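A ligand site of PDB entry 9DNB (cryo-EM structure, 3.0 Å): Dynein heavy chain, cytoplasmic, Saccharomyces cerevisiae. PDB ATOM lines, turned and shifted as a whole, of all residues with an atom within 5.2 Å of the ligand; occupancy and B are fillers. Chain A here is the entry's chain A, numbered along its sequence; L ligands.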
ATOM      1  N   GLY A 829     -32.303  -4.875 -11.263  1.00  0.00           N
ATOM      2  CA  GLY A 829     -31.738  -4.781  -9.937  1.00  0.00           C
ATOM      3  C   GLY A 829     -30.322  -4.253  -9.872  1.00  0.00           C
ATOM      4  O   GLY A 829     -29.709  -4.290  -8.794  1.00  0.00           O
ATOM      5  N   PHE A 830     -29.772  -3.765 -10.979  1.00  0.00           N
ATOM      6  CA  PHE A 830     -28.419  -3.236 -10.981  1.00  0.00           C
ATOM      7  C   PHE A 830     -28.363  -1.856 -10.348  1.00  0.00           C
ATOM      8  O   PHE A 830     -29.389  -1.181 -10.165  1.00  0.00           O
ATOM      9  CB  PHE A 830     -27.865  -3.182 -12.401  1.00  0.00           C
ATOM     10  CG  PHE A 830     -27.532  -4.526 -12.977  1.00  0.00           C
ATOM     11  CD1 PHE A 830     -27.037  -5.542 -12.172  1.00  0.00           C
ATOM     12  CD2 PHE A 830     -27.717  -4.786 -14.331  1.00  0.00           C
ATOM     13  CE1 PHE A 830     -26.732  -6.776 -12.702  1.00  0.00           C
ATOM     14  CE2 PHE A 830     -27.413  -6.021 -14.861  1.00  0.00           C
ATOM     15  CZ  PHE A 830     -26.922  -7.022 -14.048  1.00  0.00           C
ATOM     16  N   SER A 831     -27.149  -1.423 -10.007  1.00  0.00           N
ATOM     17  CA  SER A 831     -26.911  -0.117  -9.423  1.00  0.00           C
ATOM     18  C   SER A 831     -26.151   0.728 -10.432  1.00  0.00           C
ATOM     19  O   SER A 831     -25.091   0.333 -10.922  1.00  0.00           O
ATOM     20  CB  SER A 831     -26.101  -0.238  -8.127  1.00  0.00           C
ATOM     21  OG  SER A 831     -24.712  -0.272  -8.397  1.00  0.00           O
ATOM     22  N   PHE A 836     -20.400   2.088 -14.097  1.00  0.00           N
ATOM     23  CA  PHE A 836     -21.345   1.274 -14.868  1.00  0.00           C
ATOM     24  C   PHE A 836     -22.049   2.123 -15.931  1.00  0.00           C
ATOM     25  O   PHE A 836     -22.176   1.700 -17.087  1.00  0.00           O
ATOM     26  CB  PHE A 836     -22.362   0.636 -13.926  1.00  0.00           C
ATOM     27  CG  PHE A 836     -23.207  -0.425 -14.568  1.00  0.00           C
ATOM     28  CD1 PHE A 836     -22.627  -1.431 -15.317  1.00  0.00           C
ATOM     29  CD2 PHE A 836     -24.581  -0.419 -14.426  1.00  0.00           C
ATOM     30  CE1 PHE A 836     -23.398  -2.409 -15.912  1.00  0.00           C
ATOM     31  CE2 PHE A 836     -25.361  -1.397 -15.015  1.00  0.00           C
ATOM     32  CZ  PHE A 836     -24.777  -2.389 -15.761  1.00  0.00           C
ATOM     33  N   LYS A 858     -11.628  -8.179 -16.301  1.00  0.00           N
ATOM     34  CA  LYS A 858     -11.465  -9.286 -15.366  1.00  0.00           C
ATOM     35  C   LYS A 858     -12.729 -10.138 -15.357  1.00  0.00           C
ATOM     36  O   LYS A 858     -13.799  -9.727 -15.807  1.00  0.00           O
ATOM     37  CB  LYS A 858     -11.160  -8.776 -13.964  1.00  0.00           C
ATOM     38  CG  LYS A 858      -9.675  -8.733 -13.628  1.00  0.00           C
ATOM     39  CD  LYS A 858      -9.434  -8.125 -12.258  1.00  0.00           C
ATOM     40  CE  LYS A 858      -9.974  -6.704 -12.174  1.00  0.00           C
ATOM     41  NZ  LYS A 858      -9.566  -6.034 -10.914  1.00  0.00           N
ATOM     42  N   ALA A 859     -12.590 -11.359 -14.836  1.00  0.00           N
ATOM     43  CA  ALA A 859     -13.755 -12.235 -14.730  1.00  0.00           C
ATOM     44  C   ALA A 859     -14.699 -11.712 -13.653  1.00  0.00           C
ATOM     45  O   ALA A 859     -14.283 -11.448 -12.523  1.00  0.00           O
ATOM     46  CB  ALA A 859     -13.314 -13.665 -14.403  1.00  0.00           C
ATOM     47  N   GLY A 860     -15.969 -11.568 -14.005  1.00  0.00           N
ATOM     48  CA  GLY A 860     -16.929 -10.972 -13.112  1.00  0.00           C
ATOM     49  C   GLY A 860     -16.896  -9.466 -13.045  1.00  0.00           C
ATOM     50  O   GLY A 860     -17.473  -8.888 -12.112  1.00  0.00           O
ATOM     51  N   CYS A 861     -16.241  -8.800 -13.994  1.00  0.00           N
ATOM     52  CA  CYS A 861     -16.132  -7.347 -13.944  1.00  0.00           C
ATOM     53  C   CYS A 861     -17.443  -6.671 -14.330  1.00  0.00           C
ATOM     54  O   CYS A 861     -17.724  -5.549 -13.894  1.00  0.00           O
ATOM     55  CB  CYS A 861     -14.998  -6.875 -14.848  1.00  0.00           C
ATOM     56  SG  CYS A 861     -15.371  -6.964 -16.604  1.00  0.00           S
ATOM     57  N   GLY A 862     -18.264  -7.337 -15.141  1.00  0.00           N
ATOM     58  CA  GLY A 862     -19.547  -6.784 -15.510  1.00  0.00           C
ATOM     59  C   GLY A 862     -19.809  -6.624 -16.993  1.00  0.00           C
ATOM     60  O   GLY A 862     -20.560  -5.744 -17.406  1.00  0.00           O
ATOM     61  N   LYS A 863     -19.163  -7.461 -17.811  1.00  0.00           N
ATOM     62  CA  LYS A 863     -19.370  -7.398 -19.257  1.00  0.00           C
ATOM     63  C   LYS A 863     -20.804  -7.759 -19.632  1.00  0.00           C
ATOM     64  O   LYS A 863     -21.479  -7.018 -20.361  1.00  0.00           O
ATOM     65  CB  LYS A 863     -18.376  -8.320 -19.956  1.00  0.00           C
ATOM     66  CG  LYS A 863     -16.919  -7.950 -19.724  1.00  0.00           C
ATOM     67  CD  LYS A 863     -15.979  -8.950 -20.379  1.00  0.00           C
ATOM     68  CE  LYS A 863     -15.961 -10.263 -19.624  1.00  0.00           C
ATOM     69  NZ  LYS A 863     -15.376 -10.121 -18.275  1.00  0.00           N
ATOM     70  N   THR A 864     -21.275  -8.909 -19.153  1.00  0.00           N
ATOM     71  CA  THR A 864     -22.631  -9.347 -19.437  1.00  0.00           C
ATOM     72  C   THR A 864     -23.647  -8.381 -18.846  1.00  0.00           C
ATOM     73  O   THR A 864     -24.645  -8.028 -19.497  1.00  0.00           O
ATOM     74  CB  THR A 864     -22.859 -10.767 -18.899  1.00  0.00           C
ATOM     75  OG1 THR A 864     -21.737 -11.589 -19.244  1.00  0.00           O
ATOM     76  CG2 THR A 864     -24.122 -11.358 -19.488  1.00  0.00           C
ATOM     77  N   ALA A 865     -23.404  -7.946 -17.613  1.00  0.00           N
ATOM     78  CA  ALA A 865     -24.266  -6.958 -16.963  1.00  0.00           C
ATOM     79  C   ALA A 865     -24.346  -5.664 -17.758  1.00  0.00           C
ATOM     80  O   ALA A 865     -25.367  -4.977 -17.708  1.00  0.00           O
ATOM     81  CB  ALA A 865     -23.765  -6.672 -15.552  1.00  0.00           C
ATOM     82  N   THR A 866     -23.292  -5.320 -18.488  1.00  0.00           N
ATOM     83  CA  THR A 866     -23.299  -4.131 -19.335  1.00  0.00           C
ATOM     84  C   THR A 866     -24.108  -4.351 -20.608  1.00  0.00           C
ATOM     85  O   THR A 866     -25.051  -3.601 -20.880  1.00  0.00           O
ATOM     86  CB  THR A 866     -21.860  -3.730 -19.680  1.00  0.00           C
ATOM     87  OG1 THR A 866     -21.214  -3.206 -18.515  1.00  0.00           O
ATOM     88  CG2 THR A 866     -21.844  -2.666 -20.776  1.00  0.00           C
ATOM     89  N   ASP A 938     -19.158 -15.958 -25.912  1.00  0.00           N
ATOM     90  CA  ASP A 938     -18.735 -15.881 -24.507  1.00  0.00           C
ATOM     91  C   ASP A 938     -17.724 -16.997 -24.215  1.00  0.00           C
ATOM     92  O   ASP A 938     -18.002 -17.963 -23.508  1.00  0.00           O
ATOM     93  CB  ASP A 938     -19.948 -15.963 -23.591  1.00  0.00           C
ATOM     94  CG  ASP A 938     -19.659 -15.478 -22.190  1.00  0.00           C
ATOM     95  OD1 ASP A 938     -18.475 -15.308 -21.840  1.00  0.00           O
ATOM     96  OD2 ASP A 938     -20.617 -15.265 -21.424  1.00  0.00           O
ATOM     97  N   GLU A 978     -17.098 -11.682 -25.772  1.00  0.00           N
ATOM     98  CA  GLU A 978     -16.948 -11.581 -24.322  1.00  0.00           C
ATOM     99  C   GLU A 978     -15.795 -12.479 -23.896  1.00  0.00           C
ATOM    100  O   GLU A 978     -15.878 -13.711 -24.032  1.00  0.00           O
ATOM    101  CB  GLU A 978     -18.245 -11.977 -23.615  1.00  0.00           C
ATOM    102  CG  GLU A 978     -18.266 -11.669 -22.125  1.00  0.00           C
ATOM    103  CD  GLU A 978     -19.625 -11.903 -21.504  1.00  0.00           C
ATOM    104  OE1 GLU A 978     -20.635 -11.544 -22.138  1.00  0.00           O
ATOM    105  OE2 GLU A 978     -19.683 -12.448 -20.379  1.00  0.00           O
ATOM    106  N   ASP A 980     -11.729 -12.413 -21.382  1.00  0.00           N
ATOM    107  CA  ASP A 980     -10.940 -11.801 -20.313  1.00  0.00           C
ATOM    108  C   ASP A 980      -9.587 -11.298 -20.787  1.00  0.00           C
ATOM    109  O   ASP A 980      -9.180 -10.194 -20.407  1.00  0.00           O
ATOM    110  CB  ASP A 980     -10.728 -12.787 -19.161  1.00  0.00           C
ATOM    111  CG  ASP A 980     -12.002 -13.073 -18.402  1.00  0.00           C
ATOM    112  OD1 ASP A 980     -12.886 -12.188 -18.364  1.00  0.00           O
ATOM    113  OD2 ASP A 980     -12.110 -14.173 -17.832  1.00  0.00           O
ATOM    114  N   VAL A1002     -17.417  -2.749 -12.460  1.00  0.00           N
ATOM    115  CA  VAL A1002     -18.419  -1.702 -12.621  1.00  0.00           C
ATOM    116  C   VAL A1002     -19.348  -1.581 -11.425  1.00  0.00           C
ATOM    117  O   VAL A1002     -20.278  -0.759 -11.452  1.00  0.00           O
ATOM    118  CB  VAL A1002     -19.289  -1.955 -13.873  1.00  0.00           C
ATOM    119  CG1 VAL A1002     -18.431  -1.934 -15.124  1.00  0.00           C
ATOM    120  CG2 VAL A1002     -20.034  -3.274 -13.744  1.00  0.00           C
ATOM    121  N   CYS A1003     -19.123  -2.369 -10.378  1.00  0.00           N
ATOM    122  CA  CYS A1003     -20.027  -2.421  -9.239  1.00  0.00           C
ATOM    123  C   CYS A1003     -19.255  -2.370  -7.930  1.00  0.00           C
ATOM    124  O   CYS A1003     -18.175  -2.965  -7.819  1.00  0.00           O
ATOM    125  CB  CYS A1003     -20.874  -3.703  -9.295  1.00  0.00           C
ATOM    126  SG  CYS A1003     -22.156  -3.780  -8.037  1.00  0.00           S
ATOM    127  N   SER A1007     -23.182  -2.704  -3.496  1.00  0.00           N
ATOM    128  CA  SER A1007     -24.167  -2.740  -4.576  1.00  0.00           C
ATOM    129  C   SER A1007     -24.310  -4.152  -5.131  1.00  0.00           C
ATOM    130  O   SER A1007     -25.427  -4.590  -5.425  1.00  0.00           O
ATOM    131  CB  SER A1007     -23.776  -1.751  -5.673  1.00  0.00           C
ATOM    132  OG  SER A1007     -23.750  -0.423  -5.178  1.00  0.00           O
ATOM    133  N   LYS A1008     -23.197  -4.872  -5.276  1.00  0.00           N
ATOM    134  CA  LYS A1008     -23.270  -6.271  -5.695  1.00  0.00           C
ATOM    135  C   LYS A1008     -23.976  -7.123  -4.650  1.00  0.00           C
ATOM    136  O   LYS A1008     -24.753  -8.019  -4.994  1.00  0.00           O
ATOM    137  CB  LYS A1008     -21.868  -6.812  -5.983  1.00  0.00           C
ATOM    138  CG  LYS A1008     -21.816  -8.327  -6.182  1.00  0.00           C
ATOM    139  CD  LYS A1008     -20.743  -8.725  -7.167  1.00  0.00           C
ATOM    140  CE  LYS A1008     -20.733 -10.229  -7.399  1.00  0.00           C
ATOM    141  NZ  LYS A1008     -22.065 -10.749  -7.783  1.00  0.00           N
ATOM    142  N   HIS A1011     -27.640  -6.443  -5.092  1.00  0.00           N
ATOM    143  CA  HIS A1011     -28.173  -7.062  -6.300  1.00  0.00           C
ATOM    144  C   HIS A1011     -28.364  -8.557  -6.120  1.00  0.00           C
ATOM    145  O   HIS A1011     -29.399  -9.121  -6.485  1.00  0.00           O
ATOM    146  CB  HIS A1011     -27.243  -6.790  -7.485  1.00  0.00           C
ATOM    147  CG  HIS A1011     -27.597  -7.580  -8.707  1.00  0.00           C
ATOM    148  ND1 HIS A1011     -26.902  -8.708  -9.091  1.00  0.00           N
ATOM    149  CD2 HIS A1011     -28.580  -7.420  -9.628  1.00  0.00           C
ATOM    150  CE1 HIS A1011     -27.439  -9.206 -10.196  1.00  0.00           C
ATOM    151  NE2 HIS A1011     -28.457  -8.436 -10.539  1.00  0.00           N
ATOM    152  N   LEU A1012     -27.369  -9.230  -5.538  1.00  0.00           N
ATOM    153  CA  LEU A1012     -27.518 -10.660  -5.263  1.00  0.00           C
ATOM    154  C   LEU A1012     -28.662 -10.905  -4.290  1.00  0.00           C
ATOM    155  O   LEU A1012     -29.450 -11.850  -4.461  1.00  0.00           O
ATOM    156  CB  LEU A1012     -26.203 -11.229  -4.716  1.00  0.00           C
ATOM    157  CG  LEU A1012     -25.018 -11.185  -5.672  1.00  0.00           C
ATOM    158  CD1 LEU A1012     -23.721 -11.371  -4.904  1.00  0.00           C
ATOM    159  CD2 LEU A1012     -25.155 -12.254  -6.756  1.00  0.00           C
ATOM    160  N   LYS A1015     -32.079 -10.222  -6.065  1.00  0.00           N
ATOM    161  CA  LYS A1015     -32.263 -11.305  -7.028  1.00  0.00           C
ATOM    162  C   LYS A1015     -32.709 -12.581  -6.339  1.00  0.00           C
ATOM    163  O   LYS A1015     -33.605 -13.289  -6.830  1.00  0.00           O
ATOM    164  CB  LYS A1015     -30.965 -11.536  -7.806  1.00  0.00           C
ATOM    165  CG  LYS A1015     -31.076 -12.590  -8.890  1.00  0.00           C
ATOM    166  CD  LYS A1015     -29.744 -12.801  -9.595  1.00  0.00           C
ATOM    167  CE  LYS A1015     -28.899 -13.842  -8.885  1.00  0.00           C
ATOM    168  NZ  LYS A1015     -27.641 -14.135  -9.638  1.00  0.00           N
ATOM    169  N   PHE A1064     -14.596 -10.312  -4.579  1.00  0.00           N
ATOM    170  CA  PHE A1064     -15.751  -9.783  -5.302  1.00  0.00           C
ATOM    171  C   PHE A1064     -16.627 -10.910  -5.842  1.00  0.00           C
ATOM    172  O   PHE A1064     -17.849 -10.793  -5.885  1.00  0.00           O
ATOM    173  CB  PHE A1064     -15.265  -8.877  -6.437  1.00  0.00           C
ATOM    174  CG  PHE A1064     -16.344  -8.017  -7.026  1.00  0.00           C
ATOM    175  CD1 PHE A1064     -16.804  -6.907  -6.355  1.00  0.00           C
ATOM    176  CD2 PHE A1064     -16.867  -8.302  -8.274  1.00  0.00           C
ATOM    177  CE1 PHE A1064     -17.786  -6.102  -6.906  1.00  0.00           C
ATOM    178  CE2 PHE A1064     -17.854  -7.502  -8.832  1.00  0.00           C
ATOM    179  CZ  PHE A1064     -18.308  -6.396  -8.149  1.00  0.00           C
ATOM    180  N   GLU A1068     -21.547 -14.070  -4.130  1.00  0.00           N
ATOM    181  CA  GLU A1068     -22.649 -14.905  -4.606  1.00  0.00           C
ATOM    182  C   GLU A1068     -22.926 -16.035  -3.620  1.00  0.00           C
ATOM    183  O   GLU A1068     -23.979 -16.062  -2.981  1.00  0.00           O
ATOM    184  CB  GLU A1068     -22.323 -15.463  -5.994  1.00  0.00           C
ATOM    185  CG  GLU A1068     -22.052 -14.387  -7.037  1.00  0.00           C
ATOM    186  CD  GLU A1068     -21.316 -14.932  -8.246  1.00  0.00           C
ATOM    187  OE1 GLU A1068     -20.714 -16.029  -8.140  1.00  0.00           O
ATOM    188  OE2 GLU A1068     -21.331 -14.263  -9.305  1.00  0.00           O
ATOM    189  N   ARG A1290     -18.851 -24.527 -17.171  1.00  0.00           N
ATOM    190  CA  ARG A1290     -19.263 -23.171 -16.834  1.00  0.00           C
ATOM    191  C   ARG A1290     -20.459 -22.729 -17.667  1.00  0.00           C
ATOM    192  O   ARG A1290     -21.266 -21.917 -17.200  1.00  0.00           O
ATOM    193  CB  ARG A1290     -18.086 -22.200 -16.981  1.00  0.00           C
ATOM    194  CG  ARG A1290     -17.806 -21.720 -18.390  1.00  0.00           C
ATOM    195  CD  ARG A1290     -16.933 -20.479 -18.380  1.00  0.00           C
ATOM    196  NE  ARG A1290     -17.693 -19.284 -18.022  1.00  0.00           N
ATOM    197  CZ  ARG A1290     -18.134 -18.381 -18.887  1.00  0.00           C
ATOM    198  NH1 ARG A1290     -17.896 -18.510 -20.186  1.00  0.00           N
ATOM    199  NH2 ARG A1290     -18.824 -17.340 -18.453  1.00  0.00           N
ATOM    200  N   GLU A1294     -23.622 -21.477 -15.588  1.00  0.00           N
ATOM    201  CA  GLU A1294     -24.020 -20.081 -15.774  1.00  0.00           C
ATOM    202  C   GLU A1294     -25.261 -19.953 -16.650  1.00  0.00           C
ATOM    203  O   GLU A1294     -26.136 -19.130 -16.362  1.00  0.00           O
ATOM    204  CB  GLU A1294     -22.860 -19.286 -16.368  1.00  0.00           C
ATOM    205  CG  GLU A1294     -23.119 -17.786 -16.441  1.00  0.00           C
ATOM    206  CD  GLU A1294     -21.971 -17.030 -17.085  1.00  0.00           C
ATOM    207  OE1 GLU A1294     -21.093 -17.674 -17.689  1.00  0.00           O
ATOM    208  OE2 GLU A1294     -21.952 -15.781 -16.983  1.00  0.00           O
ATOM    209  N   ARG A1332     -13.509 -17.651 -14.710  1.00  0.00           N
ATOM    210  CA  ARG A1332     -14.924 -17.743 -15.075  1.00  0.00           C
ATOM    211  C   ARG A1332     -15.530 -19.068 -14.628  1.00  0.00           C
ATOM    212  O   ARG A1332     -16.738 -19.142 -14.384  1.00  0.00           O
ATOM    213  CB  ARG A1332     -15.077 -17.563 -16.577  1.00  0.00           C
ATOM    214  CG  ARG A1332     -14.110 -16.561 -17.171  1.00  0.00           C
ATOM    215  CD  ARG A1332     -14.303 -16.400 -18.675  1.00  0.00           C
ATOM    216  NE  ARG A1332     -15.247 -15.329 -18.984  1.00  0.00           N
ATOM    217  CZ  ARG A1332     -15.672 -15.054 -20.214  1.00  0.00           C
ATOM    218  NH1 ARG A1332     -15.257 -15.729 -21.262  1.00  0.00           N
ATOM    219  NH2 ARG A1332     -16.547 -14.059 -20.385  1.00  0.00           N
ATOM    220  N   ARG A1335     -15.724 -18.869 -10.556  1.00  0.00           N
ATOM    221  CA  ARG A1335     -16.619 -17.825 -10.095  1.00  0.00           C
ATOM    222  C   ARG A1335     -17.992 -18.371  -9.744  1.00  0.00           C
ATOM    223  O   ARG A1335     -18.614 -17.899  -8.782  1.00  0.00           O
ATOM    224  CB  ARG A1335     -16.743 -16.742 -11.176  1.00  0.00           C
ATOM    225  CG  ARG A1335     -17.475 -15.493 -10.722  1.00  0.00           C
ATOM    226  CD  ARG A1335     -17.331 -14.375 -11.733  1.00  0.00           C
ATOM    227  NE  ARG A1335     -17.967 -14.692 -13.008  1.00  0.00           N
ATOM    228  CZ  ARG A1335     -19.240 -14.475 -13.282  1.00  0.00           C
ATOM    229  NH1 ARG A1335     -20.064 -13.953 -12.379  1.00  0.00           N
ATOM    230  NH2 ARG A1335     -19.714 -14.784 -14.480  1.00  0.00           N
ATOM    231  N   HIS A1336     -18.476 -19.364 -10.481  1.00  0.00           N
ATOM    232  CA  HIS A1336     -19.793 -19.948 -10.265  1.00  0.00           C
ATOM    233  C   HIS A1336     -19.779 -21.125  -9.309  1.00  0.00           C
ATOM    234  O   HIS A1336     -20.835 -21.727  -9.081  1.00  0.00           O
ATOM    235  CB  HIS A1336     -20.410 -20.384 -11.600  1.00  0.00           C
ATOM    236  CG  HIS A1336     -20.437 -19.307 -12.634  1.00  0.00           C
ATOM    237  ND1 HIS A1336     -19.517 -19.224 -13.653  1.00  0.00           N
ATOM    238  CD2 HIS A1336     -21.281 -18.261 -12.805  1.00  0.00           C
ATOM    239  CE1 HIS A1336     -19.789 -18.186 -14.419  1.00  0.00           C
ATOM    240  NE2 HIS A1336     -20.851 -17.583 -13.923  1.00  0.00           N
HETATM  241  P1  LIG L   1     -17.233 -13.579 -16.580  1.00  0.00           P
HETATM  242  O1  LIG L   1     -16.365 -13.301 -17.754  1.00  0.00           O
HETATM  243  O2  LIG L   1     -18.366 -14.565 -16.874  1.00  0.00           O
HETATM  244  O3  LIG L   1     -16.469 -14.055 -15.343  1.00  0.00           O
HETATM  245  P2  LIG L   1     -19.124 -11.276 -16.579  1.00  0.00           P
HETATM  246  O4  LIG L   1     -18.596  -9.988 -17.072  1.00  0.00           O
HETATM  247  O5  LIG L   1     -19.998 -12.049 -17.558  1.00  0.00           O
HETATM  248  O6  LIG L   1     -17.974 -12.250 -16.101  1.00  0.00           O
HETATM  249  P3  LIG L   1     -21.338 -10.419 -14.820  1.00  0.00           P
HETATM  250  O7  LIG L   1     -22.434 -11.406 -14.731  1.00  0.00           O
HETATM  251  O8  LIG L   1     -21.591  -9.280 -15.796  1.00  0.00           O
HETATM  252  O9  LIG L   1     -19.974 -11.093 -15.243  1.00  0.00           O
HETATM  253  O10 LIG L   1     -21.002  -9.807 -13.407  1.00  0.00           O
HETATM  254  C1  LIG L   1     -20.790 -10.644 -12.253  1.00  0.00           C
HETATM  255  C2  LIG L   1     -21.730 -10.167 -11.177  1.00  0.00           C
HETATM  256  O11 LIG L   1     -21.545  -8.743 -11.011  1.00  0.00           O
HETATM  257  C3  LIG L   1     -23.205 -10.340 -11.506  1.00  0.00           C
HETATM  258  O12 LIG L   1     -23.677 -11.591 -11.046  1.00  0.00           O
HETATM  259  C4  LIG L   1     -23.878  -9.177 -10.752  1.00  0.00           C
HETATM  260  O13 LIG L   1     -24.476  -9.608  -9.541  1.00  0.00           O
HETATM  261  C5  LIG L   1     -22.728  -8.194 -10.469  1.00  0.00           C
HETATM  262  N1  LIG L   1     -22.911  -6.874 -11.048  1.00  0.00           N
HETATM  263  C6  LIG L   1     -22.314  -6.379 -12.177  1.00  0.00           C
HETATM  264  N2  LIG L   1     -22.662  -5.158 -12.477  1.00  0.00           N
HETATM  265  C7  LIG L   1     -23.556  -4.812 -11.472  1.00  0.00           C
HETATM  266  C8  LIG L   1     -24.298  -3.644 -11.217  1.00  0.00           C
HETATM  267  N3  LIG L   1     -24.244  -2.549 -11.978  1.00  0.00           N
HETATM  268  N4  LIG L   1     -25.098  -3.629 -10.136  1.00  0.00           N
HETATM  269  C9  LIG L   1     -25.161  -4.722  -9.370  1.00  0.00           C
HETATM  270  N5  LIG L   1     -24.514  -5.882  -9.512  1.00  0.00           N
HETATM  271  C10 LIG L   1     -23.730  -5.864 -10.589  1.00  0.00           C
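OG1 of Thr 864 is in hydrogen-bond range of OE2 of Glu 978, 2.5 Å away. OE2 of Glu 978 lies within salt-bridge range of NH2 of Arg 1332. The guanidinium group of Arg 1332 lies within salt-bridge range of the side-chain carboxylate of Asp 980. NZ of Lys 863 lies within salt-bridge range of OD1 of Asp 980, 3.2 Å away. The side-chain amino group of Lys 863 is in hydrogen-bond range of the side-chain sulfur of Cys 861 (3.6 Å). NZ of Lys 863 sits at hydrogen-bond distance from O of Lys 858 (3.0 Å). OE2 of Glu 1294 is in salt-bridge range of NH2 of Arg 1335 (3.5 Å). O of Gly 862 is in hydrogen-bond range of OG1 of Thr 866, at 2.8 Å.
Phe 830 touches the ligand. Phe 836 touches the ligand (CD2 to N3, 3.3 Å). Ala 859 touches the ligand. Asp 980 touches the ligand (OD1 to O1, 3.7 Å). Val 1002 touches the ligand. Ser 1007 touches the ligand (O to C9, 3.96 Å). Leu 1012 touches the ligand. Glu 1068 touches the ligand. OE2 of Glu 1294 touches O2 of the ligand, 3.8 Å away. Of the 30 residues printed, 22 come within 4 Å of the ligand.
N of Thr 864 sits at hydrogen-bond distance from O8 of the ligand. OG1 of Thr 864 sits at hydrogen-bond distance from O5 of the ligand, at 2.5 Å. The guanidinium group (NE) of Arg 1332 lies within salt-bridge range of an oxygen (O1) of the ligand (2.6 Å). ND1 of His 1011 lies within hydrogen-bond range of O13 of the ligand, at 2.6 Å. N of Lys 863 is in hydrogen-bond range of O4 of the ligand (2.7 Å). The side-chain amino group of Lys 863 is in salt-bridge range of an oxygen (O1) of the ligand (3.4 Å). O2 of the ligand is in salt-bridge range of NH2 of Arg 1335, at 2.8 Å. The side-chain carboxylate (OE2) of Glu 978 lies close to an oxygen (O5) of the ligand, 2.9 Å away. The backbone NH (N) of Gly 860 is in hydrogen-bond range of an oxygen (O3) of the ligand (2.9 Å). The backbone NH of Ala 865 lies within hydrogen-bond range of an oxygen (O8) of the ligand (2.9 Å). The backbone NH (N) of Ser 831 is in hydrogen-bond range of a nitrogen (N4) of the ligand (3.0 Å). O of Ser 831 is in hydrogen-bond range of N3 of the ligand (3.2 Å). NZ of Lys 1008 sits at hydrogen-bond distance from O13 of the ligand, at 3.2 Å. The guanidinium group of Arg 1290 is in salt-bridge range of an oxygen (O2) of the ligand, 3.2 Å away. The backbone NH (N) of Gly 862 is in hydrogen-bond range of an oxygen (O4) of the ligand (3.3 Å). A nitrogen (N5) of the ligand lies close to the side-chain sulfur (SG) of Cys 1003.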
